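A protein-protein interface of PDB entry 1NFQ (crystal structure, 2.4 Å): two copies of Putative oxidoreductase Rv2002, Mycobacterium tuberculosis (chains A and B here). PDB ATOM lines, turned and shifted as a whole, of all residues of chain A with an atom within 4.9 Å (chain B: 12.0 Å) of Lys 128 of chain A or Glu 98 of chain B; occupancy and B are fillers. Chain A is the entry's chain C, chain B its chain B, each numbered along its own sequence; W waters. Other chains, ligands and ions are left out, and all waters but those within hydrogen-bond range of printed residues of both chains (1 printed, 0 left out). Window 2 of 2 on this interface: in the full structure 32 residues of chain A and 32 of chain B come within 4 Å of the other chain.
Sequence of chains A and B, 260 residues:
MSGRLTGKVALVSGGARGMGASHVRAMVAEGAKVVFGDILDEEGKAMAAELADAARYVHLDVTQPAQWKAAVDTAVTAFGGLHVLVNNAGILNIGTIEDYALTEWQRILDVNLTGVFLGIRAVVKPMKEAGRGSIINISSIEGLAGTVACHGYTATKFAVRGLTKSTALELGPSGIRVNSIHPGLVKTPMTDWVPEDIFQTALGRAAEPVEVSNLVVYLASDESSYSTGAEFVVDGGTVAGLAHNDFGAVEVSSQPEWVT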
ATOM      1  N   ARG A 121     -21.268  -5.508  19.873  1.00  0.00           N
ATOM      2  CA  ARG A 121     -22.248  -6.392  20.500  1.00  0.00           C
ATOM      3  C   ARG A 121     -23.062  -7.123  19.446  1.00  0.00           C
ATOM      4  O   ARG A 121     -23.397  -8.288  19.613  1.00  0.00           O
ATOM      5  CB  ARG A 121     -23.210  -5.603  21.396  1.00  0.00           C
ATOM      6  CG  ARG A 121     -22.562  -4.946  22.595  1.00  0.00           C
ATOM      7  CD  ARG A 121     -23.562  -4.091  23.384  1.00  0.00           C
ATOM      8  NE  ARG A 121     -24.445  -4.870  24.256  1.00  0.00           N
ATOM      9  CZ  ARG A 121     -25.753  -5.020  24.065  1.00  0.00           C
ATOM     10  NH1 ARG A 121     -26.357  -4.449  23.026  1.00  0.00           N
ATOM     11  NH2 ARG A 121     -26.464  -5.732  24.929  1.00  0.00           N
ATOM     12  N   VAL A 124     -20.726 -10.130  17.505  1.00  0.00           N
ATOM     13  CA  VAL A 124     -20.077 -11.226  18.214  1.00  0.00           C
ATOM     14  C   VAL A 124     -20.734 -12.590  18.033  1.00  0.00           C
ATOM     15  O   VAL A 124     -20.037 -13.597  17.916  1.00  0.00           O
ATOM     16  CB  VAL A 124     -19.949 -10.939  19.733  1.00  0.00           C
ATOM     17  CG1 VAL A 124     -19.046  -9.740  19.958  1.00  0.00           C
ATOM     18  CG2 VAL A 124     -21.313 -10.702  20.337  1.00  0.00           C
ATOM     19  N   LYS A 125     -22.061 -12.633  18.007  1.00  0.00           N
ATOM     20  CA  LYS A 125     -22.761 -13.909  17.859  1.00  0.00           C
ATOM     21  C   LYS A 125     -22.357 -14.663  16.590  1.00  0.00           C
ATOM     22  O   LYS A 125     -21.867 -15.789  16.668  1.00  0.00           O
ATOM     23  CB  LYS A 125     -24.279 -13.701  17.892  1.00  0.00           C
ATOM     24  CG  LYS A 125     -25.067 -14.996  17.985  1.00  0.00           C
ATOM     25  CD  LYS A 125     -26.561 -14.724  18.115  1.00  0.00           C
ATOM     26  CE  LYS A 125     -27.367 -16.015  18.255  1.00  0.00           C
ATOM     27  NZ  LYS A 125     -27.246 -16.893  17.053  1.00  0.00           N
ATOM     28  N   PRO A 126     -22.561 -14.060  15.405  1.00  0.00           N
ATOM     29  CA  PRO A 126     -22.172 -14.772  14.182  1.00  0.00           C
ATOM     30  C   PRO A 126     -20.670 -15.077  14.090  1.00  0.00           C
ATOM     31  O   PRO A 126     -20.274 -16.127  13.579  1.00  0.00           O
ATOM     32  CB  PRO A 126     -22.662 -13.845  13.065  1.00  0.00           C
ATOM     33  CG  PRO A 126     -22.686 -12.500  13.704  1.00  0.00           C
ATOM     34  CD  PRO A 126     -23.224 -12.786  15.076  1.00  0.00           C
ATOM     35  N   MET A 127     -19.837 -14.167  14.587  1.00  0.00           N
ATOM     36  CA  MET A 127     -18.396 -14.386  14.557  1.00  0.00           C
ATOM     37  C   MET A 127     -17.984 -15.527  15.479  1.00  0.00           C
ATOM     38  O   MET A 127     -17.124 -16.328  15.122  1.00  0.00           O
ATOM     39  CB  MET A 127     -17.638 -13.117  14.956  1.00  0.00           C
ATOM     40  CG  MET A 127     -17.678 -12.014  13.916  1.00  0.00           C
ATOM     41  SD  MET A 127     -16.530 -10.661  14.318  1.00  0.00           S
ATOM     42  CE  MET A 127     -16.790  -9.583  12.926  1.00  0.00           C
ATOM     43  N   LYS A 128     -18.585 -15.603  16.662  1.00  0.00           N
ATOM     44  CA  LYS A 128     -18.252 -16.668  17.599  1.00  0.00           C
ATOM     45  C   LYS A 128     -18.661 -18.034  17.054  1.00  0.00           C
ATOM     46  O   LYS A 128     -18.014 -19.045  17.340  1.00  0.00           O
ATOM     47  CB  LYS A 128     -18.929 -16.441  18.953  1.00  0.00           C
ATOM     48  CG  LYS A 128     -18.234 -15.441  19.850  1.00  0.00           C
ATOM     49  CD  LYS A 128     -18.815 -15.484  21.254  1.00  0.00           C
ATOM     50  CE  LYS A 128     -17.968 -14.671  22.219  1.00  0.00           C
ATOM     51  NZ  LYS A 128     -18.437 -14.783  23.627  1.00  0.00           N
ATOM     52  N   GLU A 129     -19.735 -18.068  16.271  1.00  0.00           N
ATOM     53  CA  GLU A 129     -20.201 -19.327  15.702  1.00  0.00           C
ATOM     54  C   GLU A 129     -19.249 -19.766  14.604  1.00  0.00           C
ATOM     55  O   GLU A 129     -18.968 -20.955  14.455  1.00  0.00           O
ATOM     56  CB  GLU A 129     -21.614 -19.180  15.131  1.00  0.00           C
ATOM     57  CG  GLU A 129     -22.659 -18.752  16.152  1.00  0.00           C
ATOM     58  CD  GLU A 129     -24.068 -18.762  15.583  1.00  0.00           C
ATOM     59  OE1 GLU A 129     -24.236 -18.369  14.407  1.00  0.00           O
ATOM     60  OE2 GLU A 129     -25.009 -19.149  16.312  1.00  0.00           O
ATOM     61  N   ALA A 130     -18.757 -18.798  13.836  1.00  0.00           N
ATOM     62  CA  ALA A 130     -17.821 -19.074  12.754  1.00  0.00           C
ATOM     63  C   ALA A 130     -16.436 -19.402  13.320  1.00  0.00           C
ATOM     64  O   ALA A 130     -15.591 -19.973  12.629  1.00  0.00           O
ATOM     65  CB  ALA A 130     -17.739 -17.875  11.812  1.00  0.00           C
ATOM     66  N   GLY A 131     -16.205 -19.035  14.578  1.00  0.00           N
ATOM     67  CA  GLY A 131     -14.926 -19.316  15.211  1.00  0.00           C
ATOM     68  C   GLY A 131     -13.746 -18.459  14.780  1.00  0.00           C
ATOM     69  O   GLY A 131     -12.609 -18.730  15.163  1.00  0.00           O
ATOM     70  N   GLU A 170     -11.192 -10.186  25.773  1.00  0.00           N
ATOM     71  CA  GLU A 170     -12.354 -11.022  26.008  1.00  0.00           C
ATOM     72  C   GLU A 170     -12.680 -11.940  24.836  1.00  0.00           C
ATOM     73  O   GLU A 170     -13.012 -13.103  25.035  1.00  0.00           O
ATOM     74  CB  GLU A 170     -13.570 -10.145  26.333  1.00  0.00           C
ATOM     75  CG  GLU A 170     -14.817 -10.925  26.712  1.00  0.00           C
ATOM     76  CD  GLU A 170     -15.930 -10.028  27.212  1.00  0.00           C
ATOM     77  OE1 GLU A 170     -15.705  -9.307  28.206  1.00  0.00           O
ATOM     78  OE2 GLU A 170     -17.029 -10.042  26.614  1.00  0.00           O
ATOM     79  N   LEU A 171     -12.574 -11.419  23.618  1.00  0.00           N
ATOM     80  CA  LEU A 171     -12.902 -12.193  22.427  1.00  0.00           C
ATOM     81  C   LEU A 171     -11.771 -13.054  21.870  1.00  0.00           C
ATOM     82  O   LEU A 171     -12.018 -13.940  21.042  1.00  0.00           O
ATOM     83  CB  LEU A 171     -13.414 -11.256  21.326  1.00  0.00           C
ATOM     84  CG  LEU A 171     -14.646 -10.412  21.675  1.00  0.00           C
ATOM     85  CD1 LEU A 171     -14.965  -9.476  20.521  1.00  0.00           C
ATOM     86  CD2 LEU A 171     -15.832 -11.315  21.981  1.00  0.00           C
ATOM     87  N   SER A 174     -12.119 -16.776  21.537  1.00  0.00           N
ATOM     88  CA  SER A 174     -13.095 -17.220  20.540  1.00  0.00           C
ATOM     89  C   SER A 174     -12.570 -17.084  19.123  1.00  0.00           C
ATOM     90  O   SER A 174     -13.303 -17.328  18.160  1.00  0.00           O
ATOM     91  CB  SER A 174     -14.391 -16.420  20.658  1.00  0.00           C
ATOM     92  OG  SER A 174     -15.012 -16.641  21.908  1.00  0.00           O
ATOM     93  N   ILE A 176     -11.513 -14.245  17.758  1.00  0.00           N
ATOM     94  CA  ILE A 176     -11.853 -12.946  17.197  1.00  0.00           C
ATOM     95  C   ILE A 176     -10.802 -11.899  17.557  1.00  0.00           C
ATOM     96  O   ILE A 176     -10.436 -11.743  18.718  1.00  0.00           O
ATOM     97  CB  ILE A 176     -13.226 -12.479  17.704  1.00  0.00           C
ATOM     98  CG1 ILE A 176     -14.296 -13.496  17.289  1.00  0.00           C
ATOM     99  CG2 ILE A 176     -13.536 -11.095  17.157  1.00  0.00           C
ATOM    100  CD1 ILE A 176     -15.649 -13.263  17.930  1.00  0.00           C
ATOM    101  N   ILE B  94     -19.283  -4.220  36.009  1.00  0.00           N
ATOM    102  CA  ILE B  94     -18.623  -5.162  35.119  1.00  0.00           C
ATOM    103  C   ILE B  94     -19.614  -5.974  34.298  1.00  0.00           C
ATOM    104  O   ILE B  94     -20.818  -5.903  34.514  1.00  0.00           O
ATOM    105  CB  ILE B  94     -17.714  -6.125  35.922  1.00  0.00           C
ATOM    106  CG1 ILE B  94     -18.562  -6.991  36.859  1.00  0.00           C
ATOM    107  CG2 ILE B  94     -16.701  -5.327  36.743  1.00  0.00           C
ATOM    108  CD1 ILE B  94     -17.751  -7.986  37.677  1.00  0.00           C
ATOM    109  N   GLY B  95     -19.091  -6.743  33.350  1.00  0.00           N
ATOM    110  CA  GLY B  95     -19.937  -7.568  32.510  1.00  0.00           C
ATOM    111  C   GLY B  95     -19.321  -7.827  31.148  1.00  0.00           C
ATOM    112  O   GLY B  95     -18.579  -7.001  30.629  1.00  0.00           O
ATOM    113  N   THR B  96     -19.631  -8.973  30.557  1.00  0.00           N
ATOM    114  CA  THR B  96     -19.104  -9.313  29.244  1.00  0.00           C
ATOM    115  C   THR B  96     -19.912  -8.604  28.169  1.00  0.00           C
ATOM    116  O   THR B  96     -21.043  -8.173  28.411  1.00  0.00           O
ATOM    117  CB  THR B  96     -19.171 -10.832  28.993  1.00  0.00           C
ATOM    118  OG1 THR B  96     -20.534 -11.267  29.047  1.00  0.00           O
ATOM    119  CG2 THR B  96     -18.377 -11.577  30.044  1.00  0.00           C
ATOM    120  N   ILE B  97     -19.324  -8.483  26.983  1.00  0.00           N
ATOM    121  CA  ILE B  97     -19.974  -7.832  25.847  1.00  0.00           C
ATOM    122  C   ILE B  97     -21.439  -8.246  25.680  1.00  0.00           C
ATOM    123  O   ILE B  97     -22.294  -7.415  25.388  1.00  0.00           O
ATOM    124  CB  ILE B  97     -19.227  -8.156  24.524  1.00  0.00           C
ATOM    125  CG1 ILE B  97     -17.758  -7.766  24.654  1.00  0.00           C
ATOM    126  CG2 ILE B  97     -19.846  -7.396  23.359  1.00  0.00           C
ATOM    127  CD1 ILE B  97     -16.939  -8.086  23.429  1.00  0.00           C
ATOM    128  N   GLU B  98     -21.728  -9.528  25.873  1.00  0.00           N
ATOM    129  CA  GLU B  98     -23.088 -10.027  25.705  1.00  0.00           C
ATOM    130  C   GLU B  98     -24.091  -9.678  26.797  1.00  0.00           C
ATOM    131  O   GLU B  98     -25.150  -9.128  26.500  1.00  0.00           O
ATOM    132  CB  GLU B  98     -23.079 -11.549  25.510  1.00  0.00           C
ATOM    133  CG  GLU B  98     -22.530 -11.991  24.173  1.00  0.00           C
ATOM    134  CD  GLU B  98     -21.123 -12.533  24.279  1.00  0.00           C
ATOM    135  OE1 GLU B  98     -20.290 -11.897  24.957  1.00  0.00           O
ATOM    136  OE2 GLU B  98     -20.851 -13.594  23.677  1.00  0.00           O
ATOM    137  N   ASP B  99     -23.776  -9.998  28.049  1.00  0.00           N
ATOM    138  CA  ASP B  99     -24.703  -9.721  29.136  1.00  0.00           C
ATOM    139  C   ASP B  99     -24.439  -8.444  29.940  1.00  0.00           C
ATOM    140  O   ASP B  99     -24.683  -8.393  31.143  1.00  0.00           O
ATOM    141  CB  ASP B  99     -24.779 -10.941  30.061  1.00  0.00           C
ATOM    142  CG  ASP B  99     -23.426 -11.366  30.577  1.00  0.00           C
ATOM    143  OD1 ASP B  99     -23.308 -12.508  31.072  1.00  0.00           O
ATOM    144  OD2 ASP B  99     -22.481 -10.553  30.494  1.00  0.00           O
ATOM    145  N   TYR B 100     -23.952  -7.410  29.264  1.00  0.00           N
ATOM    146  CA  TYR B 100     -23.683  -6.124  29.899  1.00  0.00           C
ATOM    147  C   TYR B 100     -24.826  -5.206  29.476  1.00  0.00           C
ATOM    148  O   TYR B 100     -24.973  -4.897  28.295  1.00  0.00           O
ATOM    149  CB  TYR B 100     -22.346  -5.566  29.414  1.00  0.00           C
ATOM    150  CG  TYR B 100     -21.894  -4.294  30.103  1.00  0.00           C
ATOM    151  CD1 TYR B 100     -21.695  -4.250  31.487  1.00  0.00           C
ATOM    152  CD2 TYR B 100     -21.617  -3.150  29.365  1.00  0.00           C
ATOM    153  CE1 TYR B 100     -21.225  -3.093  32.113  1.00  0.00           C
ATOM    154  CE2 TYR B 100     -21.148  -1.992  29.979  1.00  0.00           C
ATOM    155  CZ  TYR B 100     -20.952  -1.967  31.348  1.00  0.00           C
ATOM    156  OH  TYR B 100     -20.478  -0.817  31.938  1.00  0.00           O
ATOM    157  N   ALA B 101     -25.637  -4.785  30.443  1.00  0.00           N
ATOM    158  CA  ALA B 101     -26.795  -3.938  30.176  1.00  0.00           C
ATOM    159  C   ALA B 101     -26.456  -2.569  29.603  1.00  0.00           C
ATOM    160  O   ALA B 101     -25.531  -1.899  30.060  1.00  0.00           O
ATOM    161  CB  ALA B 101     -27.620  -3.774  31.456  1.00  0.00           C
ATOM    162  N   LEU B 102     -27.217  -2.152  28.599  1.00  0.00           N
ATOM    163  CA  LEU B 102     -26.993  -0.857  27.981  1.00  0.00           C
ATOM    164  C   LEU B 102     -27.185   0.267  28.986  1.00  0.00           C
ATOM    165  O   LEU B 102     -26.612   1.346  28.834  1.00  0.00           O
ATOM    166  CB  LEU B 102     -27.932  -0.659  26.789  1.00  0.00           C
ATOM    167  CG  LEU B 102     -27.633  -1.555  25.584  1.00  0.00           C
ATOM    168  CD1 LEU B 102     -28.604  -1.242  24.461  1.00  0.00           C
ATOM    169  CD2 LEU B 102     -26.196  -1.332  25.121  1.00  0.00           C
ATOM    170  N   THR B 103     -27.991   0.016  30.014  1.00  0.00           N
ATOM    171  CA  THR B 103     -28.236   1.024  31.038  1.00  0.00           C
ATOM    172  C   THR B 103     -27.018   1.183  31.942  1.00  0.00           C
ATOM    173  O   THR B 103     -26.742   2.281  32.411  1.00  0.00           O
ATOM    174  CB  THR B 103     -29.476   0.681  31.901  1.00  0.00           C
ATOM    175  OG1 THR B 103     -29.372  -0.659  32.397  1.00  0.00           O
ATOM    176  CG2 THR B 103     -30.749   0.828  31.081  1.00  0.00           C
ATOM    177  N   GLU B 104     -26.292   0.092  32.189  1.00  0.00           N
ATOM    178  CA  GLU B 104     -25.088   0.161  33.015  1.00  0.00           C
ATOM    179  C   GLU B 104     -24.024   0.914  32.218  1.00  0.00           C
ATOM    180  O   GLU B 104     -23.246   1.688  32.775  1.00  0.00           O
ATOM    181  CB  GLU B 104     -24.558  -1.229  33.348  1.00  0.00           C
ATOM    182  CG  GLU B 104     -25.510  -2.132  34.111  1.00  0.00           C
ATOM    183  CD  GLU B 104     -24.876  -3.492  34.425  1.00  0.00           C
ATOM    184  OE1 GLU B 104     -24.051  -3.568  35.367  1.00  0.00           O
ATOM    185  OE2 GLU B 104     -25.185  -4.484  33.718  1.00  0.00           O
ATOM    186  N   TRP B 105     -24.003   0.675  30.908  1.00  0.00           N
ATOM    187  CA  TRP B 105     -23.061   1.330  30.011  1.00  0.00           C
ATOM    188  C   TRP B 105     -23.287   2.841  30.031  1.00  0.00           C
ATOM    189  O   TRP B 105     -22.338   3.611  30.162  1.00  0.00           O
ATOM    190  CB  TRP B 105     -23.229   0.779  28.589  1.00  0.00           C
ATOM    191  CG  TRP B 105     -22.592   1.604  27.504  1.00  0.00           C
ATOM    192  CD1 TRP B 105     -23.196   2.569  26.748  1.00  0.00           C
ATOM    193  CD2 TRP B 105     -21.230   1.536  27.051  1.00  0.00           C
ATOM    194  NE1 TRP B 105     -22.301   3.103  25.853  1.00  0.00           N
ATOM    195  CE2 TRP B 105     -21.085   2.489  26.017  1.00  0.00           C
ATOM    196  CE3 TRP B 105     -20.119   0.762  27.418  1.00  0.00           C
ATOM    197  CZ2 TRP B 105     -19.874   2.691  25.344  1.00  0.00           C
ATOM    198  CZ3 TRP B 105     -18.909   0.962  26.747  1.00  0.00           C
ATOM    199  CH2 TRP B 105     -18.800   1.920  25.721  1.00  0.00           C
ATOM    200  N   THR B 147      -8.917  -4.861  30.247  1.00  0.00           N
ATOM    201  CA  THR B 147      -9.279  -5.912  31.188  1.00  0.00           C
ATOM    202  C   THR B 147     -10.554  -6.561  30.662  1.00  0.00           C
ATOM    203  O   THR B 147     -11.425  -5.881  30.112  1.00  0.00           O
ATOM    204  CB  THR B 147      -9.574  -5.337  32.591  1.00  0.00           C
ATOM    205  OG1 THR B 147      -8.405  -4.688  33.100  1.00  0.00           O
ATOM    206  CG2 THR B 147      -9.982  -6.442  33.547  1.00  0.00           C
ATOM    207  N   VAL B 148     -10.658  -7.873  30.824  1.00  0.00           N
ATOM    208  CA  VAL B 148     -11.834  -8.604  30.378  1.00  0.00           C
ATOM    209  C   VAL B 148     -13.074  -8.177  31.174  1.00  0.00           C
ATOM    210  O   VAL B 148     -12.986  -7.898  32.374  1.00  0.00           O
ATOM    211  CB  VAL B 148     -11.628 -10.121  30.558  1.00  0.00           C
ATOM    212  CG1 VAL B 148     -12.915 -10.862  30.249  1.00  0.00           C
ATOM    213  CG2 VAL B 148     -10.521 -10.605  29.642  1.00  0.00           C
ATOM    214  N   ALA B 149     -14.219  -8.120  30.490  1.00  0.00           N
ATOM    215  CA  ALA B 149     -15.496  -7.761  31.107  1.00  0.00           C
ATOM    216  C   ALA B 149     -15.486  -6.424  31.834  1.00  0.00           C
ATOM    217  O   ALA B 149     -16.218  -6.233  32.806  1.00  0.00           O
ATOM    218  CB  ALA B 149     -15.931  -8.869  32.074  1.00  0.00           C
ATOM    219  N   CYS B 150     -14.680  -5.492  31.347  1.00  0.00           N
ATOM    220  CA  CYS B 150     -14.555  -4.182  31.977  1.00  0.00           C
ATOM    221  C   CYS B 150     -14.612  -3.086  30.908  1.00  0.00           C
ATOM    222  O   CYS B 150     -13.864  -2.108  30.953  1.00  0.00           O
ATOM    223  CB  CYS B 150     -13.214  -4.136  32.701  1.00  0.00           C
ATOM    224  SG  CYS B 150     -13.230  -3.273  34.244  1.00  0.00           S
ATOM    225  N   HIS B 151     -15.519  -3.256  29.957  1.00  0.00           N
ATOM    226  CA  HIS B 151     -15.664  -2.341  28.835  1.00  0.00           C
ATOM    227  C   HIS B 151     -16.091  -0.905  29.139  1.00  0.00           C
ATOM    228  O   HIS B 151     -15.515   0.041  28.599  1.00  0.00           O
ATOM    229  CB  HIS B 151     -16.592  -3.000  27.820  1.00  0.00           C
ATOM    230  CG  HIS B 151     -16.248  -4.434  27.573  1.00  0.00           C
ATOM    231  ND1 HIS B 151     -15.038  -4.820  27.038  1.00  0.00           N
ATOM    232  CD2 HIS B 151     -16.899  -5.578  27.893  1.00  0.00           C
ATOM    233  CE1 HIS B 151     -14.956  -6.139  27.043  1.00  0.00           C
ATOM    234  NE2 HIS B 151     -16.073  -6.623  27.557  1.00  0.00           N
ATOM    235  N   GLY B 152     -17.091  -0.731  29.993  1.00  0.00           N
ATOM    236  CA  GLY B 152     -17.527   0.612  30.324  1.00  0.00           C
ATOM    237  C   GLY B 152     -16.460   1.355  31.106  1.00  0.00           C
ATOM    238  O   GLY B 152     -16.122   2.498  30.802  1.00  0.00           O
HETATM  239  O   HOH W   1     -17.796 -12.448  25.612  1.00  0.00           O
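No position is printed for both chains. Of the 11 pairs that touch across the chains among the printed residues, none has its exchanged pair printed and touching as well.
The side-chain carboxylate (OE2) of Glu 98 of chain B lies within salt-bridge range of the side-chain amino group (NZ) of Lys 128 of chain A, at 2.7 Å. The backbone NH (N) of Ala 149 of chain B sits at hydrogen-bond distance from the side-chain carboxylate (OE1) of Glu 170 of chain A (3.0 Å). A ring nitrogen (NE2) of His 151 of chain B lies within hydrogen-bond range of the side-chain carboxylate (OE1) of Glu 170 of chain A. The backbone NH (N) of Ile 97 of chain B sits at hydrogen-bond distance from the side-chain carboxylate (OE2) of Glu 170 of chain A (2.8 Å).
Of the printed residues of chain B, Lys 128 of chain A touches Glu 98. Of chain A, only Arg 121 and Lys 128 come within 4 Å of Glu 98 of chain B. Arg 121 of chain A touches just these residues of chain B: Ile 97, Glu 98, Tyr 100 and Leu 102. No residue of chain B comes within 4 Å of Val 124 of chain A. No residue of chain B comes within 4 Å of Pro 126 of chain A. No residue of chain B comes within 4 Å of Met 127 of chain A. No residue of chain B comes within 4 Å of Glu 129 of chain A. No residue of chain B comes within 4 Å of Ala 130 of chain A. No residue of chain B comes within 4 Å of Gly 131 of chain A. Of chain B, only Ile 97 comes within 4 Å of Leu 171 of chain A. Ser 174 of chain A touches none of the printed residues of chain B. Of the printed residues of chain A, Ala 149 of chain B touches Glu 170 (3.0 Å). Of the printed residues of chain A, Ile 97 of chain B touches Arg 121, Glu 170 and Leu 171. Of the printed residues of chain A, Val 148 of chain B touches Glu 170 (3.8 Å). Printed residues of chain A within 4 Å of Leu 102 of chain B: Arg 121. Ala 101 of chain B touches none of the printed residues of chain A. Thr 103 of chain B touches none of the printed residues of chain A. The nearest printed residue of chain B that does not touch Lys 128 of chain A is Thr 96 of chain B (6.7 Å). The nearest printed residue of chain A that does not touch Thr 96 of chain B is Arg 121 of chain A (6.3 Å).
Among the printed residues, merely in contact across the chains: Glu 170 of chain A with Thr 96 of chain B (3.3 Å), Arg 121 of chain A with Ile 97 of chain B (3.5 Å), Leu 171 of chain A with Ile 97 of chain B (3.7 Å), Arg 121 of chain A with Leu 102 of chain B (3.8 Å), Arg 121 of chain A with Tyr 100 of chain B (3.8 Å), Glu 170 of chain A with Val 148 of chain B (3.8 Å) and Arg 121 of chain A with Glu 98 of chain B (3.97 Å).
Water W1 lies within hydrogen-bond range of OE1 of Glu 98 of chain B (2.6 Å), OE2 of Glu 170 of chain A (2.7 Å) and NZ of Lys 128 of chain A (3.1 Å).
Printed residues of chain B that touch a printed residue of chain A: Thr 96, Ile 97, Glu 98, Tyr 100, Leu 102, Val 148, Ala 149 and His 151. Hydrophobic or aromatic side chains of chain B within 4 Å of the printed part of chain A: Ile 97, Leu 102, Val 148, Ala 149 and His 151. Among the printed residues, Asp or Glu carboxylates within 4 Å of a Lys or Arg side-chain nitrogen of the other chain: Lys 128 of chain A with Glu 98 of chain B (2.7 Å).
The side-chain hydroxyl of Thr 96 of chain B lies within hydrogen-bond range of the side-chain carboxylate of Asp 99 of chain B (2.5 Å). The backbone carbonyl oxygen (O) of Leu 171 of chain A sits at hydrogen-bond distance from the backbone NH (N) of Ile 176 of chain A (3.3 Å). O of Ala 149 of chain B is in hydrogen-bond range of N of Gly 95 of chain B (3.0 Å).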
